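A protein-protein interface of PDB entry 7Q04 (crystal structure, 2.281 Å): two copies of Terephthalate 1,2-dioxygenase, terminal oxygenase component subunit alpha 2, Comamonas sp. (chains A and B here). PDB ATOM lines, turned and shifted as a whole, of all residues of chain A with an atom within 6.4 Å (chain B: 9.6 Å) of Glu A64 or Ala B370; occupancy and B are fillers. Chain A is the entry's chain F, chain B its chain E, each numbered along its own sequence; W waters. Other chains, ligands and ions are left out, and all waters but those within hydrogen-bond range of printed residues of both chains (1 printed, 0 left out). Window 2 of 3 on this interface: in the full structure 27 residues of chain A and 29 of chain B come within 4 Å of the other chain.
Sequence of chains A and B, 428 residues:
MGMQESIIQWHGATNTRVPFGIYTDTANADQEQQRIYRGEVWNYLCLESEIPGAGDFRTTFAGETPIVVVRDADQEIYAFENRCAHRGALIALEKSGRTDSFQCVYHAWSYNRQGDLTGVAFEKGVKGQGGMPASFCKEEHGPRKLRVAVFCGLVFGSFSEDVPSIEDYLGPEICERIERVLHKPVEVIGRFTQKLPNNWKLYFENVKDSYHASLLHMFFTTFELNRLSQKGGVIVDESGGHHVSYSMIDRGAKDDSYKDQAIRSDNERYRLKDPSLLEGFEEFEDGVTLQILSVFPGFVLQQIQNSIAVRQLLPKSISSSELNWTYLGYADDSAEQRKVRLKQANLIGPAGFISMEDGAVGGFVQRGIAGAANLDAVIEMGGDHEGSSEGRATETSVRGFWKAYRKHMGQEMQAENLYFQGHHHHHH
Water W1 lies within hydrogen-bond range of the backbone NH (N) of Gly B371 (2.8 Å), the side-chain carboxylate (OE2) of Glu A81 (2.8 Å) and the backbone carbonyl oxygen (O) of Gly B368 (2.9 Å).
No residue of chain B comes within 4 Å of Gly A63.
Of chain B, only Gly B371 (3.5 Å) comes within 4 Å of Thr A65.
Printed residues of chain B within 4 Å of Arg A83: Gly B368 (3.4 Å), Ala B372 (3.4 Å) and Leu B375 (3.2 Å).
Printed residues of chain A within 4 Å of Gly B368: Arg A83.
Printed residues of chain A within 4 Å of Gly B371: Arg A38 (3.5 Å), Glu A64 (3.6 Å) and Thr A65 (3.5 Å).
Of the printed residues of chain A, Ala B372 touches Arg A83.
Of the printed residues of chain A, Leu B375 touches Arg A83.
N of Phe B20 sits at hydrogen-bond distance from O of Leu B375.
OE1 of Gln A33 sits at hydrogen-bond distance from N of Glu A64, at 2.9 Å.
O of Gln A33 lies within hydrogen-bond range of N of Arg A38 (3.0 Å).
The side-chain carboxylate (OE2) of Glu A81 is in salt-bridge range of the guanidinium group (NE) of Arg A83.
OG1 of Thr A65 is in hydrogen-bond range of NH2 of Arg A38 (3.3 Å).
NH2 of Arg A38 is in salt-bridge range of OE2 of Glu A64, 2.9 Å away.
The backbone carbonyl oxygen of Ala B370 sits close to the side-chain carboxylate of Glu A64, 3.4 Å away.
Arg A38 touches Gly B371.
Glu A64 touches Gly B371.
Gly B371 touches Thr A65 (CA to OG1, 3.5 Å).
Gly B368 touches Arg A83 (O to CB, 3.4 Å).
Arg A83 touches Ala B372.
Arg A83 touches Leu B375 (NH1 to CD1, 3.2 Å).
No position is printed for both chains.
Of the 7 pairs that touch across the chains among the printed residues, none has its exchanged pair printed and touching as well.
Hydrophobic or aromatic side chains of chain B that line the printed part of chain A: Ala B370, Ala B372 and Leu B375.
Of the 15 printed residues of chain A, 4 touch a printed residue of chain B.
Printed residues of chain A that touch a printed residue of chain B: Arg A38, Glu A64, Thr A65 and Arg A83.
Among the printed residues, 7 pairs touch across the chains.
Among the printed residues, no Asp or Glu carboxylate lies within 4 Å of a Lys or Arg side-chain nitrogen of the other chain.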
ATOM      1  N   ALA A  29     -20.709 -25.191   4.478  1.00  0.00           N
ATOM      2  CA  ALA A  29     -19.704 -24.130   4.231  1.00  0.00           C
ATOM      3  C   ALA A  29     -18.720 -24.117   5.396  1.00  0.00           C
ATOM      4  O   ALA A  29     -17.500 -24.000   5.144  1.00  0.00           O
ATOM      5  CB  ALA A  29     -20.349 -22.777   4.029  1.00  0.00           C
ATOM      6  N   ASP A  30     -19.226 -24.239   6.629  1.00  0.00           N
ATOM      7  CA  ASP A  30     -18.353 -24.184   7.824  1.00  0.00           C
ATOM      8  C   ASP A  30     -17.439 -25.432   7.777  1.00  0.00           C
ATOM      9  O   ASP A  30     -16.249 -25.299   8.063  1.00  0.00           O
ATOM     10  CB  ASP A  30     -19.209 -23.897   9.059  1.00  0.00           C
ATOM     11  CG  ASP A  30     -18.397 -23.689  10.323  1.00  0.00           C
ATOM     12  OD1 ASP A  30     -17.244 -23.190  10.254  1.00  0.00           O
ATOM     13  OD2 ASP A  30     -18.933 -24.026  11.378  1.00  0.00           O
ATOM     14  N   GLN A  33     -14.529 -24.699   5.573  1.00  0.00           N
ATOM     15  CA  GLN A  33     -13.486 -23.945   6.311  1.00  0.00           C
ATOM     16  C   GLN A  33     -12.579 -24.936   7.049  1.00  0.00           C
ATOM     17  O   GLN A  33     -11.352 -24.836   6.886  1.00  0.00           O
ATOM     18  CB  GLN A  33     -14.107 -22.911   7.243  1.00  0.00           C
ATOM     19  CG  GLN A  33     -14.949 -21.863   6.512  1.00  0.00           C
ATOM     20  CD  GLN A  33     -14.164 -21.048   5.508  1.00  0.00           C
ATOM     21  OE1 GLN A  33     -12.956 -20.852   5.618  1.00  0.00           O
ATOM     22  NE2 GLN A  33     -14.854 -20.579   4.484  1.00  0.00           N
ATOM     23  N   GLN A  34     -13.148 -25.888   7.790  1.00  0.00           N
ATOM     24  CA  GLN A  34     -12.369 -26.824   8.644  1.00  0.00           C
ATOM     25  C   GLN A  34     -11.604 -27.813   7.757  1.00  0.00           C
ATOM     26  O   GLN A  34     -10.433 -28.065   8.026  1.00  0.00           O
ATOM     27  CB  GLN A  34     -13.278 -27.579   9.614  1.00  0.00           C
ATOM     28  CG  GLN A  34     -13.746 -26.697  10.762  1.00  0.00           C
ATOM     29  CD  GLN A  34     -14.999 -27.182  11.445  1.00  0.00           C
ATOM     30  OE1 GLN A  34     -16.003 -26.482  11.512  1.00  0.00           O
ATOM     31  NE2 GLN A  34     -14.939 -28.378  12.005  1.00  0.00           N
ATOM     32  N   TYR A  37     -10.074 -25.269   3.588  1.00  0.00           N
ATOM     33  CA  TYR A  37      -9.178 -24.087   3.648  1.00  0.00           C
ATOM     34  C   TYR A  37      -8.116 -24.294   4.738  1.00  0.00           C
ATOM     35  O   TYR A  37      -6.921 -24.016   4.466  1.00  0.00           O
ATOM     36  CB  TYR A  37     -10.026 -22.813   3.733  1.00  0.00           C
ATOM     37  CG  TYR A  37     -10.804 -22.499   2.474  1.00  0.00           C
ATOM     38  CD1 TYR A  37     -10.171 -22.095   1.306  1.00  0.00           C
ATOM     39  CD2 TYR A  37     -12.189 -22.593   2.458  1.00  0.00           C
ATOM     40  CE1 TYR A  37     -10.901 -21.810   0.160  1.00  0.00           C
ATOM     41  CE2 TYR A  37     -12.929 -22.335   1.320  1.00  0.00           C
ATOM     42  CZ  TYR A  37     -12.288 -21.929   0.159  1.00  0.00           C
ATOM     43  OH  TYR A  37     -13.030 -21.627  -0.964  1.00  0.00           O
ATOM     44  N   ARG A  38      -8.509 -24.814   5.910  1.00  0.00           N
ATOM     45  CA  ARG A  38      -7.568 -25.170   7.004  1.00  0.00           C
ATOM     46  C   ARG A  38      -7.259 -26.684   6.996  1.00  0.00           C
ATOM     47  O   ARG A  38      -6.802 -27.207   8.029  1.00  0.00           O
ATOM     48  CB  ARG A  38      -8.128 -24.711   8.354  1.00  0.00           C
ATOM     49  CG  ARG A  38      -8.559 -23.249   8.424  1.00  0.00           C
ATOM     50  CD  ARG A  38      -8.729 -22.734   9.848  1.00  0.00           C
ATOM     51  NE  ARG A  38      -9.926 -23.262  10.501  1.00  0.00           N
ATOM     52  CZ  ARG A  38     -11.164 -22.817  10.338  1.00  0.00           C
ATOM     53  NH1 ARG A  38     -12.160 -23.395  10.976  1.00  0.00           N
ATOM     54  NH2 ARG A  38     -11.430 -21.805   9.534  1.00  0.00           N
ATOM     55  N   PHE A  61      -6.294 -13.791   2.978  1.00  0.00           N
ATOM     56  CA  PHE A  61      -7.206 -14.783   3.579  1.00  0.00           C
ATOM     57  C   PHE A  61      -6.793 -16.175   3.103  1.00  0.00           C
ATOM     58  O   PHE A  61      -6.239 -16.324   2.009  1.00  0.00           O
ATOM     59  CB  PHE A  61      -8.643 -14.392   3.215  1.00  0.00           C
ATOM     60  CG  PHE A  61      -9.218 -13.260   4.038  1.00  0.00           C
ATOM     61  CD1 PHE A  61      -9.829 -13.511   5.262  1.00  0.00           C
ATOM     62  CD2 PHE A  61      -9.194 -11.955   3.562  1.00  0.00           C
ATOM     63  CE1 PHE A  61     -10.383 -12.477   6.020  1.00  0.00           C
ATOM     64  CE2 PHE A  61      -9.755 -10.916   4.305  1.00  0.00           C
ATOM     65  CZ  PHE A  61     -10.350 -11.173   5.537  1.00  0.00           C
ATOM     66  N   ALA A  62      -7.022 -17.152   3.958  1.00  0.00           N
ATOM     67  CA  ALA A  62      -7.139 -18.575   3.593  1.00  0.00           C
ATOM     68  C   ALA A  62      -8.542 -18.994   4.030  1.00  0.00           C
ATOM     69  O   ALA A  62      -8.776 -19.172   5.257  1.00  0.00           O
ATOM     70  CB  ALA A  62      -6.042 -19.394   4.244  1.00  0.00           C
ATOM     71  N   GLY A  63      -9.438 -19.110   3.064  1.00  0.00           N
ATOM     72  CA  GLY A  63     -10.886 -19.147   3.313  1.00  0.00           C
ATOM     73  C   GLY A  63     -11.329 -17.933   4.091  1.00  0.00           C
ATOM     74  O   GLY A  63     -10.905 -16.816   3.710  1.00  0.00           O
ATOM     75  N   GLU A  64     -12.111 -18.160   5.152  1.00  0.00           N
ATOM     76  CA  GLU A  64     -12.647 -17.098   6.053  1.00  0.00           C
ATOM     77  C   GLU A  64     -11.489 -16.475   6.870  1.00  0.00           C
ATOM     78  O   GLU A  64     -11.689 -15.392   7.458  1.00  0.00           O
ATOM     79  CB  GLU A  64     -13.751 -17.691   6.954  1.00  0.00           C
ATOM     80  CG  GLU A  64     -13.252 -18.694   8.041  1.00  0.00           C
ATOM     81  CD  GLU A  64     -14.337 -19.455   8.804  1.00  0.00           C
ATOM     82  OE1 GLU A  64     -15.534 -19.109   8.634  1.00  0.00           O
ATOM     83  OE2 GLU A  64     -14.003 -20.411   9.544  1.00  0.00           O
ATOM     84  N   THR A  65     -10.350 -17.164   6.984  1.00  0.00           N
ATOM     85  CA  THR A  65      -9.332 -16.892   8.033  1.00  0.00           C
ATOM     86  C   THR A  65      -8.311 -15.885   7.526  1.00  0.00           C
ATOM     87  O   THR A  65      -7.569 -16.148   6.586  1.00  0.00           O
ATOM     88  CB  THR A  65      -8.613 -18.161   8.503  1.00  0.00           C
ATOM     89  OG1 THR A  65      -9.544 -19.132   8.974  1.00  0.00           O
ATOM     90  CG2 THR A  65      -7.625 -17.858   9.596  1.00  0.00           C
ATOM     91  N   PRO A  66      -8.194 -14.714   8.162  1.00  0.00           N
ATOM     92  CA  PRO A  66      -7.227 -13.723   7.712  1.00  0.00           C
ATOM     93  C   PRO A  66      -5.798 -14.178   8.026  1.00  0.00           C
ATOM     94  O   PRO A  66      -5.618 -14.873   9.029  1.00  0.00           O
ATOM     95  CB  PRO A  66      -7.585 -12.482   8.532  1.00  0.00           C
ATOM     96  CG  PRO A  66      -8.133 -13.078   9.832  1.00  0.00           C
ATOM     97  CD  PRO A  66      -8.895 -14.315   9.388  1.00  0.00           C
ATOM     98  N   GLU A  81      -1.781 -16.831  11.030  1.00  0.00           N
ATOM     99  CA  GLU A  81      -3.158 -16.364  11.218  1.00  0.00           C
ATOM    100  C   GLU A  81      -3.099 -14.939  11.788  1.00  0.00           C
ATOM    101  O   GLU A  81      -2.348 -14.712  12.750  1.00  0.00           O
ATOM    102  CB  GLU A  81      -3.840 -17.346  12.166  1.00  0.00           C
ATOM    103  CG  GLU A  81      -5.270 -16.954  12.502  1.00  0.00           C
ATOM    104  CD  GLU A  81      -5.957 -17.994  13.362  1.00  0.00           C
ATOM    105  OE1 GLU A  81      -5.235 -18.870  13.915  1.00  0.00           O
ATOM    106  OE2 GLU A  81      -7.200 -17.949  13.462  1.00  0.00           O
ATOM    107  N   ARG A  83      -4.579 -13.100  13.928  1.00  0.00           N
ATOM    108  CA  ARG A  83      -5.415 -13.141  15.151  1.00  0.00           C
ATOM    109  C   ARG A  83      -4.515 -13.065  16.386  1.00  0.00           C
ATOM    110  O   ARG A  83      -3.706 -13.993  16.606  1.00  0.00           O
ATOM    111  CB  ARG A  83      -6.229 -14.434  15.203  1.00  0.00           C
ATOM    112  CG  ARG A  83      -6.970 -14.642  16.521  1.00  0.00           C
ATOM    113  CD  ARG A  83      -7.911 -15.835  16.439  1.00  0.00           C
ATOM    114  NE  ARG A  83      -7.193 -17.066  16.163  1.00  0.00           N
ATOM    115  CZ  ARG A  83      -6.455 -17.724  17.055  1.00  0.00           C
ATOM    116  NH1 ARG A  83      -5.812 -18.832  16.704  1.00  0.00           N
ATOM    117  NH2 ARG A  83      -6.361 -17.250  18.288  1.00  0.00           N
ATOM    118  N   PRO A 315     -13.860 -17.283  -0.588  1.00  0.00           N
ATOM    119  CA  PRO A 315     -15.261 -17.290  -0.195  1.00  0.00           C
ATOM    120  C   PRO A 315     -15.489 -16.114   0.762  1.00  0.00           C
ATOM    121  O   PRO A 315     -14.537 -15.732   1.456  1.00  0.00           O
ATOM    122  CB  PRO A 315     -15.383 -18.593   0.588  1.00  0.00           C
ATOM    123  CG  PRO A 315     -14.007 -18.703   1.249  1.00  0.00           C
ATOM    124  CD  PRO A 315     -13.043 -18.233   0.168  1.00  0.00           C
ATOM    125  N   ILE B   7     -20.011 -24.431  20.537  1.00  0.00           N
ATOM    126  CA  ILE B   7     -18.957 -23.379  20.414  1.00  0.00           C
ATOM    127  C   ILE B   7     -19.080 -22.367  21.587  1.00  0.00           C
ATOM    128  O   ILE B   7     -18.249 -21.416  21.632  1.00  0.00           O
ATOM    129  CB  ILE B   7     -19.080 -22.815  18.975  1.00  0.00           C
ATOM    130  CG1 ILE B   7     -17.715 -22.592  18.321  1.00  0.00           C
ATOM    131  CG2 ILE B   7     -20.032 -21.632  18.842  1.00  0.00           C
ATOM    132  CD1 ILE B   7     -17.279 -23.764  17.453  1.00  0.00           C
ATOM    133  N   PHE B  20     -14.776 -17.869  21.999  1.00  0.00           N
ATOM    134  CA  PHE B  20     -14.976 -16.870  20.921  1.00  0.00           C
ATOM    135  C   PHE B  20     -16.336 -17.073  20.266  1.00  0.00           C
ATOM    136  O   PHE B  20     -16.847 -16.104  19.668  1.00  0.00           O
ATOM    137  CB  PHE B  20     -13.867 -16.964  19.879  1.00  0.00           C
ATOM    138  CG  PHE B  20     -12.583 -16.293  20.290  1.00  0.00           C
ATOM    139  CD1 PHE B  20     -12.602 -15.052  20.917  1.00  0.00           C
ATOM    140  CD2 PHE B  20     -11.357 -16.862  19.983  1.00  0.00           C
ATOM    141  CE1 PHE B  20     -11.417 -14.420  21.263  1.00  0.00           C
ATOM    142  CE2 PHE B  20     -10.177 -16.232  20.333  1.00  0.00           C
ATOM    143  CZ  PHE B  20     -10.206 -15.011  20.986  1.00  0.00           C
ATOM    144  N   GLY B  21     -16.928 -18.271  20.381  1.00  0.00           N
ATOM    145  CA  GLY B  21     -18.265 -18.521  19.806  1.00  0.00           C
ATOM    146  C   GLY B  21     -19.333 -17.705  20.502  1.00  0.00           C
ATOM    147  O   GLY B  21     -20.409 -17.561  19.926  1.00  0.00           O
ATOM    148  N   TYR B  23     -19.595 -14.732  20.808  1.00  0.00           N
ATOM    149  CA  TYR B  23     -19.738 -13.494  19.998  1.00  0.00           C
ATOM    150  C   TYR B  23     -20.373 -13.761  18.624  1.00  0.00           C
ATOM    151  O   TYR B  23     -20.524 -12.782  17.858  1.00  0.00           O
ATOM    152  CB  TYR B  23     -18.359 -12.887  19.750  1.00  0.00           C
ATOM    153  CG  TYR B  23     -17.550 -12.517  20.971  1.00  0.00           C
ATOM    154  CD1 TYR B  23     -18.029 -11.667  21.956  1.00  0.00           C
ATOM    155  CD2 TYR B  23     -16.258 -13.013  21.114  1.00  0.00           C
ATOM    156  CE1 TYR B  23     -17.251 -11.327  23.056  1.00  0.00           C
ATOM    157  CE2 TYR B  23     -15.472 -12.686  22.206  1.00  0.00           C
ATOM    158  CZ  TYR B  23     -15.961 -11.829  23.171  1.00  0.00           C
ATOM    159  OH  TYR B  23     -15.090 -11.481  24.161  1.00  0.00           O
ATOM    160  N   THR B  24     -20.817 -14.999  18.370  1.00  0.00           N
ATOM    161  CA  THR B  24     -21.202 -15.548  17.042  1.00  0.00           C
ATOM    162  C   THR B  24     -22.486 -16.391  17.116  1.00  0.00           C
ATOM    163  O   THR B  24     -23.222 -16.398  16.134  1.00  0.00           O
ATOM    164  CB  THR B  24     -19.994 -16.331  16.511  1.00  0.00           C
ATOM    165  OG1 THR B  24     -19.451 -15.320  15.674  1.00  0.00           O
ATOM    166  CG2 THR B  24     -20.266 -17.640  15.781  1.00  0.00           C
ATOM    167  N   GLY B 363     -14.596  -4.390  16.336  1.00  0.00           N
ATOM    168  CA  GLY B 363     -14.633  -4.929  14.966  1.00  0.00           C
ATOM    169  C   GLY B 363     -13.384  -5.706  14.646  1.00  0.00           C
ATOM    170  O   GLY B 363     -13.492  -6.726  13.969  1.00  0.00           O
ATOM    171  N   PHE B 364     -12.239  -5.227  15.102  1.00  0.00           N
ATOM    172  CA  PHE B 364     -10.929  -5.898  14.878  1.00  0.00           C
ATOM    173  C   PHE B 364     -11.005  -7.304  15.478  1.00  0.00           C
ATOM    174  O   PHE B 364     -10.515  -8.228  14.847  1.00  0.00           O
ATOM    175  CB  PHE B 364      -9.763  -5.064  15.430  1.00  0.00           C
ATOM    176  CG  PHE B 364      -9.534  -3.746  14.733  1.00  0.00           C
ATOM    177  CD1 PHE B 364     -10.082  -3.479  13.494  1.00  0.00           C
ATOM    178  CD2 PHE B 364      -8.767  -2.764  15.323  1.00  0.00           C
ATOM    179  CE1 PHE B 364      -9.880  -2.259  12.867  1.00  0.00           C
ATOM    180  CE2 PHE B 364      -8.569  -1.541  14.700  1.00  0.00           C
ATOM    181  CZ  PHE B 364      -9.137  -1.286  13.482  1.00  0.00           C
ATOM    182  N   VAL B 365     -11.685  -7.446  16.612  1.00  0.00           N
ATOM    183  CA  VAL B 365     -11.836  -8.747  17.309  1.00  0.00           C
ATOM    184  C   VAL B 365     -12.843  -9.577  16.516  1.00  0.00           C
ATOM    185  O   VAL B 365     -12.508 -10.754  16.177  1.00  0.00           O
ATOM    186  CB  VAL B 365     -12.264  -8.590  18.778  1.00  0.00           C
ATOM    187  CG1 VAL B 365     -12.491  -9.937  19.416  1.00  0.00           C
ATOM    188  CG2 VAL B 365     -11.228  -7.819  19.573  1.00  0.00           C
ATOM    189  N   GLN B 366     -14.017  -9.003  16.247  1.00  0.00           N
ATOM    190  CA  GLN B 366     -15.064  -9.680  15.438  1.00  0.00           C
ATOM    191  C   GLN B 366     -14.421 -10.307  14.183  1.00  0.00           C
ATOM    192  O   GLN B 366     -14.737 -11.462  13.849  1.00  0.00           O
ATOM    193  CB  GLN B 366     -16.161  -8.681  15.080  1.00  0.00           C
ATOM    194  CG  GLN B 366     -17.464  -9.349  14.663  1.00  0.00           C
ATOM    195  CD  GLN B 366     -18.338  -9.760  15.824  1.00  0.00           C
ATOM    196  OE1 GLN B 366     -18.450  -9.079  16.835  1.00  0.00           O
ATOM    197  NE2 GLN B 366     -18.945 -10.918  15.700  1.00  0.00           N
ATOM    198  N   ARG B 367     -13.507  -9.591  13.526  1.00  0.00           N
ATOM    199  CA  ARG B 367     -12.902 -10.042  12.257  1.00  0.00           C
ATOM    200  C   ARG B 367     -11.710 -10.971  12.518  1.00  0.00           C
ATOM    201  O   ARG B 367     -11.552 -11.946  11.751  1.00  0.00           O
ATOM    202  CB  ARG B 367     -12.544  -8.827  11.401  1.00  0.00           C
ATOM    203  CG  ARG B 367     -13.725  -8.278  10.618  1.00  0.00           C
ATOM    204  CD  ARG B 367     -13.550  -6.819  10.267  1.00  0.00           C
ATOM    205  NE  ARG B 367     -12.377  -6.594   9.436  1.00  0.00           N
ATOM    206  CZ  ARG B 367     -11.838  -5.413   9.205  1.00  0.00           C
ATOM    207  NH1 ARG B 367     -10.753  -5.334   8.466  1.00  0.00           N
ATOM    208  NH2 ARG B 367     -12.360  -4.310   9.717  1.00  0.00           N
ATOM    209  N   GLY B 368     -10.895 -10.700  13.537  1.00  0.00           N
ATOM    210  CA  GLY B 368      -9.732 -11.537  13.874  1.00  0.00           C
ATOM    211  C   GLY B 368     -10.132 -12.978  14.196  1.00  0.00           C
ATOM    212  O   GLY B 368      -9.311 -13.916  13.953  1.00  0.00           O
ATOM    213  N   ILE B 369     -11.343 -13.180  14.719  1.00  0.00           N
ATOM    214  CA  ILE B 369     -11.759 -14.507  15.229  1.00  0.00           C
ATOM    215  C   ILE B 369     -12.552 -15.277  14.180  1.00  0.00           C
ATOM    216  O   ILE B 369     -13.125 -16.320  14.536  1.00  0.00           O
ATOM    217  CB  ILE B 369     -12.555 -14.350  16.531  1.00  0.00           C
ATOM    218  CG1 ILE B 369     -13.902 -13.655  16.303  1.00  0.00           C
ATOM    219  CG2 ILE B 369     -11.684 -13.694  17.612  1.00  0.00           C
ATOM    220  CD1 ILE B 369     -14.737 -13.549  17.556  1.00  0.00           C
ATOM    221  N   ALA B 370     -12.612 -14.780  12.948  1.00  0.00           N
ATOM    222  CA  ALA B 370     -13.480 -15.344  11.892  1.00  0.00           C
ATOM    223  C   ALA B 370     -13.249 -16.865  11.727  1.00  0.00           C
ATOM    224  O   ALA B 370     -14.226 -17.572  11.470  1.00  0.00           O
ATOM    225  CB  ALA B 370     -13.227 -14.593  10.618  1.00  0.00           C
ATOM    226  N   GLY B 371     -12.009 -17.339  11.879  1.00  0.00           N
ATOM    227  CA  GLY B 371     -11.646 -18.759  11.717  1.00  0.00           C
ATOM    228  C   GLY B 371     -11.373 -19.477  13.047  1.00  0.00           C
ATOM    229  O   GLY B 371     -10.806 -20.593  13.023  1.00  0.00           O
ATOM    230  N   ALA B 372     -11.784 -18.894  14.167  1.00  0.00           N
ATOM    231  CA  ALA B 372     -11.402 -19.310  15.531  1.00  0.00           C
ATOM    232  C   ALA B 372     -12.637 -19.360  16.425  1.00  0.00           C
ATOM    233  O   ALA B 372     -12.513 -19.027  17.618  1.00  0.00           O
ATOM    234  CB  ALA B 372     -10.390 -18.324  16.076  1.00  0.00           C
ATOM    235  N   ALA B 373     -13.784 -19.751  15.899  1.00  0.00           N
ATOM    236  CA  ALA B 373     -15.018 -19.800  16.708  1.00  0.00           C
ATOM    237  C   ALA B 373     -14.837 -20.809  17.873  1.00  0.00           C
ATOM    238  O   ALA B 373     -15.505 -20.660  18.930  1.00  0.00           O
ATOM    239  CB  ALA B 373     -16.217 -20.098  15.823  1.00  0.00           C
ATOM    240  N   ASN B 374     -13.945 -21.794  17.710  1.00  0.00           N
ATOM    241  CA  ASN B 374     -13.770 -22.932  18.670  1.00  0.00           C
ATOM    242  C   ASN B 374     -12.655 -22.633  19.674  1.00  0.00           C
ATOM    243  O   ASN B 374     -12.480 -23.465  20.579  1.00  0.00           O
ATOM    244  CB  ASN B 374     -13.474 -24.240  17.944  1.00  0.00           C
ATOM    245  CG  ASN B 374     -12.240 -24.135  17.069  1.00  0.00           C
ATOM    246  OD1 ASN B 374     -11.682 -23.051  16.806  1.00  0.00           O
ATOM    247  ND2 ASN B 374     -11.803 -25.289  16.627  1.00  0.00           N
ATOM    248  N   LEU B 375     -11.956 -21.492  19.533  1.00  0.00           N
ATOM    249  CA  LEU B 375     -10.851 -21.066  20.449  1.00  0.00           C
ATOM    250  C   LEU B 375     -11.381 -20.114  21.536  1.00  0.00           C
ATOM    251  O   LEU B 375     -12.588 -19.789  21.534  1.00  0.00           O
ATOM    252  CB  LEU B 375      -9.711 -20.471  19.606  1.00  0.00           C
ATOM    253  CG  LEU B 375      -9.185 -21.420  18.515  1.00  0.00           C
ATOM    254  CD1 LEU B 375      -8.078 -20.805  17.663  1.00  0.00           C
ATOM    255  CD2 LEU B 375      -8.681 -22.733  19.129  1.00  0.00           C
HETATM  256  O   HOH W   1      -9.528 -16.553  12.787  1.00  0.00           O
